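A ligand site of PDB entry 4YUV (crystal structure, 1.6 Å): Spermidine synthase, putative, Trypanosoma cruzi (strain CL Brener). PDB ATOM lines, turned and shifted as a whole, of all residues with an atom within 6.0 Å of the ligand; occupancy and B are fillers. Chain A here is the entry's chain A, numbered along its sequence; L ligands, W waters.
Water W1 lies within hydrogen-bond range of the side-chain carboxylate (OD2) of Asp 176, the side-chain carboxylate (OD1) of Asp 106, the backbone NH (N) of Val 109, a nitrogen (N1) of the ligand and the backbone NH (N) of Gly 108.
Leu 67 touches the ligand.
OE1 of Gln 72 touches C3 of the ligand, 3.0 Å away.
Tyr 81 touches the ligand (CE2 to C1, 3.7 Å).
CA of Gly 103 touches N5 of the ligand (3.6 Å).
Gly 104 touches the ligand (N to C6, 3.9 Å).
Val 125 touches the ligand (O to C14, 3.7 Å).
CB of Asp 128 touches O2 of the ligand, 3.5 Å away.
CG1 of Val 131 touches O3 of the ligand (3.4 Å).
Gly 156 touches the ligand.
CA of Thr 177 touches O1 of the ligand, at 3.4 Å.
Leu 187 touches the ligand.
Tyr 245 touches the ligand (OH to C1, 3.5 Å).
Hydrophobic or aromatic side chains within 4 Å of the ligand: Leu 67, Tyr 81, His 82, Ile 127, Val 131, Pro 183, Ala 184 and Leu 187.
23 residues have an atom within 4 Å of the ligand: Gln 48, Leu 67, Gln 72, Tyr 81, His 82, Gly 103, Gly 104, Asp 106, Val 125, Asp 126, Ile 127, Asp 128, Val 131, Gly 156, Asp 157, Gly 158, Asp 176, Thr 177, Thr 178, Pro 183, Ala 184, Leu 187 and Tyr 245.
Along chain A the residues within 4 Å of the ligand span positions 48 to 245.
The nearest printed residue that does not touch the ligand is Gly 105 (4.1 Å).
O2 of the ligand lies within hydrogen-bond range of OD1 of Asp 126, at 2.6 Å.
The side-chain carboxylate (OD2) of Asp 106 is in salt-bridge range of a nitrogen (N1) of the ligand.
S1 of the ligand sits close to O of Asp 176.
N1 of the ligand lies within salt-bridge range of OD2 of Asp 176, at 2.8 Å.
The side-chain carboxylate (OD1) of Asp 157 lies within hydrogen-bond range of a nitrogen (N4) of the ligand (2.9 Å).
The backbone NH (N) of Gly 158 sits at hydrogen-bond distance from a nitrogen (N6) of the ligand (2.9 Å).
A nitrogen (N1) of the ligand is in hydrogen-bond range of a ring nitrogen (NE2) of His 82, 3.0 Å away.
O of Pro 183 lies within hydrogen-bond range of N4 of the ligand (3.0 Å).
NE2 of Gln 48 sits at hydrogen-bond distance from O2 of the ligand (3.0 Å).
The backbone NH (N) of Thr 178 sits at hydrogen-bond distance from an oxygen (O1) of the ligand, 3.5 Å away.
N of Ile 127 lies within hydrogen-bond range of N5 of the ligand (3.3 Å).
The backbone NH of Ala 184 is in hydrogen-bond range of a nitrogen (N3) of the ligand (3.4 Å).
The side-chain carboxylate (OD1) of Asp 126 is in hydrogen-bond range of the backbone NH (N) of Asp 128, at 2.9 Å.
OD2 of Asp 126 is in hydrogen-bond range of N of Gly 105 (2.9 Å).
OD1 of Asp 106 lies within hydrogen-bond range of NE2 of His 82 (3.4 Å).
The side-chain carboxylate of Asp 106 lies within hydrogen-bond range of the backbone NH of Gly 108.
The backbone carbonyl oxygen of Asp 176 sits at hydrogen-bond distance from the backbone NH of Gly 104 (3.0 Å).
The side-chain hydroxyl (OH) of Tyr 245 lies within hydrogen-bond range of the backbone carbonyl oxygen (O) of Gln 72.
N of Gln 72 is in hydrogen-bond range of O of Met 65, 2.7 Å away.
The backbone NH of Ile 127 is in hydrogen-bond range of the backbone carbonyl oxygen of Gly 156, at 3.1 Å.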
ATOM      1  N   GLN A  48      11.190 -15.885   2.525  1.00  0.00           N
ATOM      2  CA  GLN A  48      11.364 -17.334   2.312  1.00  0.00           C
ATOM      3  C   GLN A  48      10.095 -18.012   1.905  1.00  0.00           C
ATOM      4  O   GLN A  48       8.994 -17.476   2.130  1.00  0.00           O
ATOM      5  CB  GLN A  48      11.828 -17.988   3.688  1.00  0.00           C
ATOM      6  CG  GLN A  48      13.160 -17.411   4.172  1.00  0.00           C
ATOM      7  CD  GLN A  48      13.482 -17.840   5.585  1.00  0.00           C
ATOM      8  OE1 GLN A  48      14.459 -18.603   5.784  1.00  0.00           O
ATOM      9  NE2 GLN A  48      12.672 -17.362   6.605  1.00  0.00           N
ATOM     10  N   MET A  65       7.610 -28.721   8.907  1.00  0.00           N
ATOM     11  CA  MET A  65       7.768 -27.364   8.463  1.00  0.00           C
ATOM     12  C   MET A  65       9.030 -27.326   7.636  1.00  0.00           C
ATOM     13  O   MET A  65      10.122 -27.760   8.047  1.00  0.00           O
ATOM     14  CB  MET A  65       7.848 -26.321   9.648  1.00  0.00           C
ATOM     15  CG  MET A  65       8.235 -24.906   9.128  1.00  0.00           C
ATOM     16  SD  MET A  65       8.837 -23.673  10.394  1.00  0.00           S
ATOM     17  CE  MET A  65       7.382 -23.597  11.333  1.00  0.00           C
ATOM     18  N   LEU A  67      11.559 -24.606   4.969  1.00  0.00           N
ATOM     19  CA  LEU A  67      11.816 -23.242   4.464  1.00  0.00           C
ATOM     20  C   LEU A  67      12.707 -23.389   3.273  1.00  0.00           C
ATOM     21  O   LEU A  67      13.762 -24.010   3.361  1.00  0.00           O
ATOM     22  CB  LEU A  67      12.502 -22.323   5.528  1.00  0.00           C
ATOM     23  CG  LEU A  67      11.647 -21.807   6.676  1.00  0.00           C
ATOM     24  CD1 LEU A  67      12.533 -21.156   7.756  1.00  0.00           C
ATOM     25  CD2 LEU A  67      10.733 -20.717   6.138  1.00  0.00           C
ATOM     26  N   GLN A  72      12.788 -28.030   8.451  1.00  0.00           N
ATOM     27  CA  GLN A  72      13.189 -27.252   9.625  1.00  0.00           C
ATOM     28  C   GLN A  72      12.831 -27.923  10.917  1.00  0.00           C
ATOM     29  O   GLN A  72      13.673 -27.979  11.832  1.00  0.00           O
ATOM     30  CB  GLN A  72      12.496 -25.871   9.630  1.00  0.00           C
ATOM     31  CG  GLN A  72      12.848 -25.025   8.402  1.00  0.00           C
ATOM     32  CD  GLN A  72      14.324 -24.667   8.363  1.00  0.00           C
ATOM     33  OE1 GLN A  72      14.845 -23.994   9.270  1.00  0.00           O
ATOM     34  NE2 GLN A  72      15.025 -25.150   7.362  1.00  0.00           N
ATOM     35  N   VAL A  73      11.562 -28.364  11.076  1.00  0.00           N
ATOM     36  CA  VAL A  73      11.118 -29.045  12.266  1.00  0.00           C
ATOM     37  C   VAL A  73      10.086 -30.143  11.902  1.00  0.00           C
ATOM     38  O   VAL A  73       9.407 -30.015  10.884  1.00  0.00           O
ATOM     39  CB  VAL A  73      10.563 -27.891  13.125  1.00  0.00           C
ATOM     40  CG1 VAL A  73       9.096 -27.535  13.032  1.00  0.00           C
ATOM     41  CG2 VAL A  73      11.389 -27.358  14.203  1.00  0.00           C
ATOM     42  N   TYR A  81      17.204 -31.319  18.399  1.00  0.00           N
ATOM     43  CA  TYR A  81      17.995 -30.167  18.138  1.00  0.00           C
ATOM     44  C   TYR A  81      17.696 -29.091  19.113  1.00  0.00           C
ATOM     45  O   TYR A  81      18.563 -28.413  19.639  1.00  0.00           O
ATOM     46  CB  TYR A  81      17.674 -29.738  16.701  1.00  0.00           C
ATOM     47  CG  TYR A  81      18.308 -28.486  16.231  1.00  0.00           C
ATOM     48  CD1 TYR A  81      19.621 -28.466  15.713  1.00  0.00           C
ATOM     49  CD2 TYR A  81      17.585 -27.337  16.282  1.00  0.00           C
ATOM     50  CE1 TYR A  81      20.179 -27.298  15.208  1.00  0.00           C
ATOM     51  CE2 TYR A  81      18.116 -26.171  15.828  1.00  0.00           C
ATOM     52  CZ  TYR A  81      19.363 -26.173  15.254  1.00  0.00           C
ATOM     53  OH  TYR A  81      19.741 -24.908  14.862  1.00  0.00           O
ATOM     54  N   HIS A  82      16.422 -29.010  19.513  1.00  0.00           N
ATOM     55  CA  HIS A  82      16.084 -27.904  20.457  1.00  0.00           C
ATOM     56  C   HIS A  82      16.684 -28.176  21.824  1.00  0.00           C
ATOM     57  O   HIS A  82      17.216 -27.273  22.460  1.00  0.00           O
ATOM     58  CB  HIS A  82      14.559 -27.804  20.506  1.00  0.00           C
ATOM     59  CG  HIS A  82      14.017 -27.270  19.221  1.00  0.00           C
ATOM     60  ND1 HIS A  82      12.814 -27.672  18.692  1.00  0.00           N
ATOM     61  CD2 HIS A  82      14.578 -26.427  18.289  1.00  0.00           C
ATOM     62  CE1 HIS A  82      12.623 -27.049  17.534  1.00  0.00           C
ATOM     63  NE2 HIS A  82      13.676 -26.293  17.268  1.00  0.00           N
ATOM     64  N   ILE A 102      19.274 -15.993  17.995  1.00  0.00           N
ATOM     65  CA  ILE A 102      19.160 -15.458  16.669  1.00  0.00           C
ATOM     66  C   ILE A 102      18.579 -16.531  15.791  1.00  0.00           C
ATOM     67  O   ILE A 102      19.012 -17.667  15.805  1.00  0.00           O
ATOM     68  CB  ILE A 102      20.576 -15.077  16.149  1.00  0.00           C
ATOM     69  CG1 ILE A 102      21.167 -13.935  17.019  1.00  0.00           C
ATOM     70  CG2 ILE A 102      20.497 -14.637  14.671  1.00  0.00           C
ATOM     71  CD1 ILE A 102      20.553 -12.571  16.889  1.00  0.00           C
ATOM     72  N   GLY A 103      17.502 -16.157  15.054  1.00  0.00           N
ATOM     73  CA  GLY A 103      16.672 -17.161  14.377  1.00  0.00           C
ATOM     74  C   GLY A 103      15.665 -17.769  15.322  1.00  0.00           C
ATOM     75  O   GLY A 103      15.161 -17.090  16.180  1.00  0.00           O
ATOM     76  N   GLY A 104      15.484 -19.039  15.189  1.00  0.00           N
ATOM     77  CA  GLY A 104      14.686 -19.729  16.182  1.00  0.00           C
ATOM     78  C   GLY A 104      13.234 -19.341  16.273  1.00  0.00           C
ATOM     79  O   GLY A 104      12.606 -19.489  17.319  1.00  0.00           O
ATOM     80  N   GLY A 105      12.679 -18.798  15.187  1.00  0.00           N
ATOM     81  CA  GLY A 105      11.322 -18.256  15.216  1.00  0.00           C
ATOM     82  C   GLY A 105      10.280 -19.311  15.506  1.00  0.00           C
ATOM     83  O   GLY A 105       9.154 -18.908  15.882  1.00  0.00           O
ATOM     84  N   ASP A 106      10.602 -20.597  15.400  1.00  0.00           N
ATOM     85  CA  ASP A 106       9.590 -21.636  15.744  1.00  0.00           C
ATOM     86  C   ASP A 106       9.375 -21.716  17.218  1.00  0.00           C
ATOM     87  O   ASP A 106       8.287 -22.183  17.664  1.00  0.00           O
ATOM     88  CB  ASP A 106      10.037 -22.984  15.232  1.00  0.00           C
ATOM     89  CG  ASP A 106      11.452 -23.257  15.560  1.00  0.00           C
ATOM     90  OD1 ASP A 106      11.710 -23.591  16.646  1.00  0.00           O
ATOM     91  OD2 ASP A 106      12.305 -23.071  14.688  1.00  0.00           O
ATOM     92  N   GLY A 108      11.353 -23.391  19.480  1.00  0.00           N
ATOM     93  CA  GLY A 108      11.806 -24.606  20.157  1.00  0.00           C
ATOM     94  C   GLY A 108      12.990 -24.395  21.074  1.00  0.00           C
ATOM     95  O   GLY A 108      13.005 -24.850  22.223  1.00  0.00           O
ATOM     96  N   VAL A 109      14.060 -23.773  20.589  1.00  0.00           N
ATOM     97  CA  VAL A 109      15.183 -23.470  21.474  1.00  0.00           C
ATOM     98  C   VAL A 109      14.764 -22.622  22.670  1.00  0.00           C
ATOM     99  O   VAL A 109      15.195 -22.827  23.808  1.00  0.00           O
ATOM    100  CB  VAL A 109      16.346 -22.766  20.683  1.00  0.00           C
ATOM    101  CG1 VAL A 109      17.422 -22.265  21.695  1.00  0.00           C
ATOM    102  CG2 VAL A 109      16.955 -23.757  19.669  1.00  0.00           C
ATOM    103  N   VAL A 125      15.372 -13.059  18.063  1.00  0.00           N
ATOM    104  CA  VAL A 125      15.349 -12.132  16.866  1.00  0.00           C
ATOM    105  C   VAL A 125      15.385 -13.012  15.619  1.00  0.00           C
ATOM    106  O   VAL A 125      16.438 -13.603  15.298  1.00  0.00           O
ATOM    107  CB  VAL A 125      16.505 -11.132  16.925  1.00  0.00           C
ATOM    108  CG1 VAL A 125      16.365 -10.150  15.713  1.00  0.00           C
ATOM    109  CG2 VAL A 125      16.471 -10.426  18.312  1.00  0.00           C
ATOM    110  N   ASP A 126      14.267 -13.100  14.880  1.00  0.00           N
ATOM    111  CA  ASP A 126      14.225 -13.869  13.649  1.00  0.00           C
ATOM    112  C   ASP A 126      13.756 -12.932  12.553  1.00  0.00           C
ATOM    113  O   ASP A 126      12.826 -12.129  12.768  1.00  0.00           O
ATOM    114  CB  ASP A 126      13.236 -15.051  13.852  1.00  0.00           C
ATOM    115  CG  ASP A 126      13.244 -16.034  12.716  1.00  0.00           C
ATOM    116  OD1 ASP A 126      13.065 -15.717  11.520  1.00  0.00           O
ATOM    117  OD2 ASP A 126      13.537 -17.249  12.923  1.00  0.00           O
ATOM    118  N   ILE A 127      14.363 -13.075  11.373  1.00  0.00           N
ATOM    119  CA  ILE A 127      14.088 -12.115  10.290  1.00  0.00           C
ATOM    120  C   ILE A 127      12.643 -12.298   9.752  1.00  0.00           C
ATOM    121  O   ILE A 127      12.073 -11.362   9.121  1.00  0.00           O
ATOM    122  CB  ILE A 127      15.123 -12.367   9.172  1.00  0.00           C
ATOM    123  CG1 ILE A 127      15.226 -11.127   8.260  1.00  0.00           C
ATOM    124  CG2 ILE A 127      14.825 -13.653   8.469  1.00  0.00           C
ATOM    125  CD1 ILE A 127      16.336 -11.287   7.240  1.00  0.00           C
ATOM    126  N   ASP A 128      12.085 -13.473   9.984  1.00  0.00           N
ATOM    127  CA  ASP A 128      10.804 -13.800   9.337  1.00  0.00           C
ATOM    128  C   ASP A 128       9.689 -13.944  10.318  1.00  0.00           C
ATOM    129  O   ASP A 128       9.547 -15.036  10.872  1.00  0.00           O
ATOM    130  CB  ASP A 128      10.989 -15.090   8.534  1.00  0.00           C
ATOM    131  CG  ASP A 128       9.960 -15.204   7.427  1.00  0.00           C
ATOM    132  OD1 ASP A 128       8.841 -14.722   7.643  1.00  0.00           O
ATOM    133  OD2 ASP A 128      10.251 -15.858   6.432  1.00  0.00           O
ATOM    134  N   VAL A 131       7.326 -17.127  10.340  1.00  0.00           N
ATOM    135  CA  VAL A 131       7.696 -18.375  10.993  1.00  0.00           C
ATOM    136  C   VAL A 131       7.090 -18.442  12.416  1.00  0.00           C
ATOM    137  O   VAL A 131       6.539 -19.474  12.794  1.00  0.00           O
ATOM    138  CB  VAL A 131       9.265 -18.492  11.057  1.00  0.00           C
ATOM    139  CG1 VAL A 131       9.652 -19.736  11.853  1.00  0.00           C
ATOM    140  CG2 VAL A 131       9.809 -18.679   9.637  1.00  0.00           C
ATOM    141  N   GLY A 156      13.384  -9.240  12.772  1.00  0.00           N
ATOM    142  CA  GLY A 156      14.495  -8.475  12.341  1.00  0.00           C
ATOM    143  C   GLY A 156      15.669  -9.309  11.970  1.00  0.00           C
ATOM    144  O   GLY A 156      15.817 -10.522  12.351  1.00  0.00           O
ATOM    145  N   ASP A 157      16.585  -8.724  11.209  1.00  0.00           N
ATOM    146  CA  ASP A 157      17.847  -9.382  10.902  1.00  0.00           C
ATOM    147  C   ASP A 157      18.792  -9.504  12.077  1.00  0.00           C
ATOM    148  O   ASP A 157      19.018  -8.542  12.816  1.00  0.00           O
ATOM    149  CB  ASP A 157      18.551  -8.642   9.749  1.00  0.00           C
ATOM    150  CG  ASP A 157      19.938  -9.110   9.545  1.00  0.00           C
ATOM    151  OD1 ASP A 157      20.223 -10.286   9.372  1.00  0.00           O
ATOM    152  OD2 ASP A 157      20.844  -8.265   9.656  1.00  0.00           O
ATOM    153  N   GLY A 158      19.320 -10.727  12.279  1.00  0.00           N
ATOM    154  CA  GLY A 158      20.213 -10.895  13.443  1.00  0.00           C
ATOM    155  C   GLY A 158      21.520 -10.195  13.320  1.00  0.00           C
ATOM    156  O   GLY A 158      22.115  -9.857  14.372  1.00  0.00           O
ATOM    157  N   LEU A 159      22.034 -10.014  12.101  1.00  0.00           N
ATOM    158  CA  LEU A 159      23.271  -9.249  11.995  1.00  0.00           C
ATOM    159  C   LEU A 159      23.125  -7.756  12.409  1.00  0.00           C
ATOM    160  O   LEU A 159      23.945  -7.257  13.238  1.00  0.00           O
ATOM    161  CB  LEU A 159      23.842  -9.442  10.593  1.00  0.00           C
ATOM    162  CG  LEU A 159      25.116  -8.561  10.361  1.00  0.00           C
ATOM    163  CD1 LEU A 159      26.300  -8.922  11.271  1.00  0.00           C
ATOM    164  CD2 LEU A 159      25.498  -8.647   8.855  1.00  0.00           C
ATOM    165  N   ASP A 176      20.311 -20.027  15.856  1.00  0.00           N
ATOM    166  CA  ASP A 176      19.535 -21.130  15.321  1.00  0.00           C
ATOM    167  C   ASP A 176      18.947 -20.716  13.978  1.00  0.00           C
ATOM    168  O   ASP A 176      17.835 -20.228  13.847  1.00  0.00           O
ATOM    169  CB  ASP A 176      18.432 -21.537  16.330  1.00  0.00           C
ATOM    170  CG  ASP A 176      17.417 -22.530  15.733  1.00  0.00           C
ATOM    171  OD1 ASP A 176      17.767 -23.190  14.737  1.00  0.00           O
ATOM    172  OD2 ASP A 176      16.296 -22.635  16.285  1.00  0.00           O
ATOM    173  N   THR A 177      19.806 -20.828  12.965  1.00  0.00           N
ATOM    174  CA  THR A 177      19.480 -20.291  11.654  1.00  0.00           C
ATOM    175  C   THR A 177      19.319 -21.360  10.563  1.00  0.00           C
ATOM    176  O   THR A 177      19.584 -22.547  10.732  1.00  0.00           O
ATOM    177  CB  THR A 177      20.572 -19.355  11.151  1.00  0.00           C
ATOM    178  OG1 THR A 177      21.697 -20.200  11.011  1.00  0.00           O
ATOM    179  CG2 THR A 177      20.860 -18.306  12.219  1.00  0.00           C
ATOM    180  N   THR A 178      18.791 -20.887   9.451  1.00  0.00           N
ATOM    181  CA  THR A 178      18.851 -21.657   8.181  1.00  0.00           C
ATOM    182  C   THR A 178      20.282 -21.728   7.649  1.00  0.00           C
ATOM    183  O   THR A 178      21.188 -21.254   8.289  1.00  0.00           O
ATOM    184  CB  THR A 178      17.829 -21.005   7.199  1.00  0.00           C
ATOM    185  OG1 THR A 178      18.058 -19.586   7.146  1.00  0.00           O
ATOM    186  CG2 THR A 178      16.377 -21.262   7.675  1.00  0.00           C
ATOM    187  N   GLY A 182      20.944 -18.840   1.981  1.00  0.00           N
ATOM    188  CA  GLY A 182      19.771 -17.940   1.897  1.00  0.00           C
ATOM    189  C   GLY A 182      19.932 -16.762   2.885  1.00  0.00           C
ATOM    190  O   GLY A 182      21.045 -16.216   3.003  1.00  0.00           O
ATOM    191  N   PRO A 183      18.818 -16.297   3.535  1.00  0.00           N
ATOM    192  CA  PRO A 183      18.924 -15.049   4.364  1.00  0.00           C
ATOM    193  C   PRO A 183      19.870 -15.134   5.567  1.00  0.00           C
ATOM    194  O   PRO A 183      20.183 -14.126   6.175  1.00  0.00           O
ATOM    195  CB  PRO A 183      17.465 -14.747   4.815  1.00  0.00           C
ATOM    196  CG  PRO A 183      16.715 -16.023   4.548  1.00  0.00           C
ATOM    197  CD  PRO A 183      17.441 -16.778   3.424  1.00  0.00           C
ATOM    198  N   ALA A 184      20.355 -16.334   5.906  1.00  0.00           N
ATOM    199  CA  ALA A 184      21.278 -16.509   7.039  1.00  0.00           C
ATOM    200  C   ALA A 184      22.726 -16.403   6.568  1.00  0.00           C
ATOM    201  O   ALA A 184      23.632 -16.566   7.393  1.00  0.00           O
ATOM    202  CB  ALA A 184      21.101 -17.826   7.797  1.00  0.00           C
ATOM    203  N   SER A 185      22.965 -16.112   5.298  1.00  0.00           N
ATOM    204  CA  SER A 185      24.378 -16.179   4.789  1.00  0.00           C
ATOM    205  C   SER A 185      25.477 -15.523   5.654  1.00  0.00           C
ATOM    206  O   SER A 185      26.544 -16.118   5.988  1.00  0.00           O
ATOM    207  CB  SER A 185      24.406 -15.523   3.392  1.00  0.00           C
ATOM    208  OG  SER A 185      25.751 -15.279   3.005  1.00  0.00           O
ATOM    209  N   LEU A 187      25.480 -14.866   8.731  1.00  0.00           N
ATOM    210  CA  LEU A 187      25.504 -15.360  10.130  1.00  0.00           C
ATOM    211  C   LEU A 187      26.466 -16.561  10.279  1.00  0.00           C
ATOM    212  O   LEU A 187      26.659 -17.106  11.376  1.00  0.00           O
ATOM    213  CB  LEU A 187      24.079 -15.681  10.616  1.00  0.00           C
ATOM    214  CG  LEU A 187      23.068 -14.519  10.469  1.00  0.00           C
ATOM    215  CD1 LEU A 187      22.793 -14.036   9.070  1.00  0.00           C
ATOM    216  CD2 LEU A 187      21.751 -14.980  11.010  1.00  0.00           C
ATOM    217  N   TYR A 245      17.115 -34.257   9.205  1.00  0.00           N
ATOM    218  CA  TYR A 245      18.050 -33.352   8.642  1.00  0.00           C
ATOM    219  C   TYR A 245      18.906 -34.122   7.671  1.00  0.00           C
ATOM    220  O   TYR A 245      18.982 -35.326   7.766  1.00  0.00           O
ATOM    221  CB  TYR A 245      18.919 -32.567   9.703  1.00  0.00           C
ATOM    222  CG  TYR A 245      18.160 -31.485  10.456  1.00  0.00           C
ATOM    223  CD1 TYR A 245      17.099 -30.782   9.872  1.00  0.00           C
ATOM    224  CD2 TYR A 245      18.555 -31.089  11.734  1.00  0.00           C
ATOM    225  CE1 TYR A 245      16.452 -29.767  10.557  1.00  0.00           C
ATOM    226  CE2 TYR A 245      17.906 -30.060  12.411  1.00  0.00           C
ATOM    227  CZ  TYR A 245      16.822 -29.431  11.855  1.00  0.00           C
ATOM    228  OH  TYR A 245      16.209 -28.432  12.611  1.00  0.00           O
HETATM  229  C1  LIG L   1      15.027 -25.421  14.023  1.00  0.00           C
HETATM  230  N1  LIG L   1      14.592 -24.482  15.111  1.00  0.00           N
HETATM  231  C2  LIG L   1      14.591 -24.845  12.690  1.00  0.00           C
HETATM  232  C3  LIG L   1      15.447 -23.713  12.207  1.00  0.00           C
HETATM  233  S1  LIG L   1      14.763 -22.009  12.606  1.00  0.00           S
HETATM  234  C4  LIG L   1      13.189 -22.250  11.679  1.00  0.00           C
HETATM  235  C5  LIG L   1      15.851 -21.063  11.421  1.00  0.00           C
HETATM  236  C6  LIG L   1      15.342 -19.635  11.377  1.00  0.00           C
HETATM  237  O1  LIG L   1      16.445 -18.825  10.945  1.00  0.00           O
HETATM  238  C7  LIG L   1      15.873 -17.577  10.536  1.00  0.00           C
HETATM  239  C8  LIG L   1      14.696 -18.129   9.650  1.00  0.00           C
HETATM  240  O2  LIG L   1      13.788 -17.063   9.378  1.00  0.00           O
HETATM  241  C9  LIG L   1      14.183 -19.308  10.412  1.00  0.00           C
HETATM  242  O3  LIG L   1      12.888 -19.122  11.088  1.00  0.00           O
HETATM  243  N2  LIG L   1      16.798 -16.692   9.846  1.00  0.00           N
HETATM  244  C10 LIG L   1      17.378 -16.865   8.596  1.00  0.00           C
HETATM  245  N3  LIG L   1      18.117 -15.802   8.390  1.00  0.00           N
HETATM  246  C11 LIG L   1      18.119 -14.952   9.454  1.00  0.00           C
HETATM  247  C12 LIG L   1      18.712 -13.736   9.776  1.00  0.00           C
HETATM  248  N4  LIG L   1      19.575 -13.067   8.905  1.00  0.00           N
HETATM  249  C13 LIG L   1      17.235 -15.493  10.369  1.00  0.00           C
HETATM  250  N5  LIG L   1      17.028 -14.973  11.565  1.00  0.00           N
HETATM  251  C14 LIG L   1      17.590 -13.779  11.795  1.00  0.00           C
HETATM  252  N6  LIG L   1      18.440 -13.144  10.927  1.00  0.00           N
HETATM  253  O   HOH W   1      14.098 -22.739  17.816  1.00  0.00           O
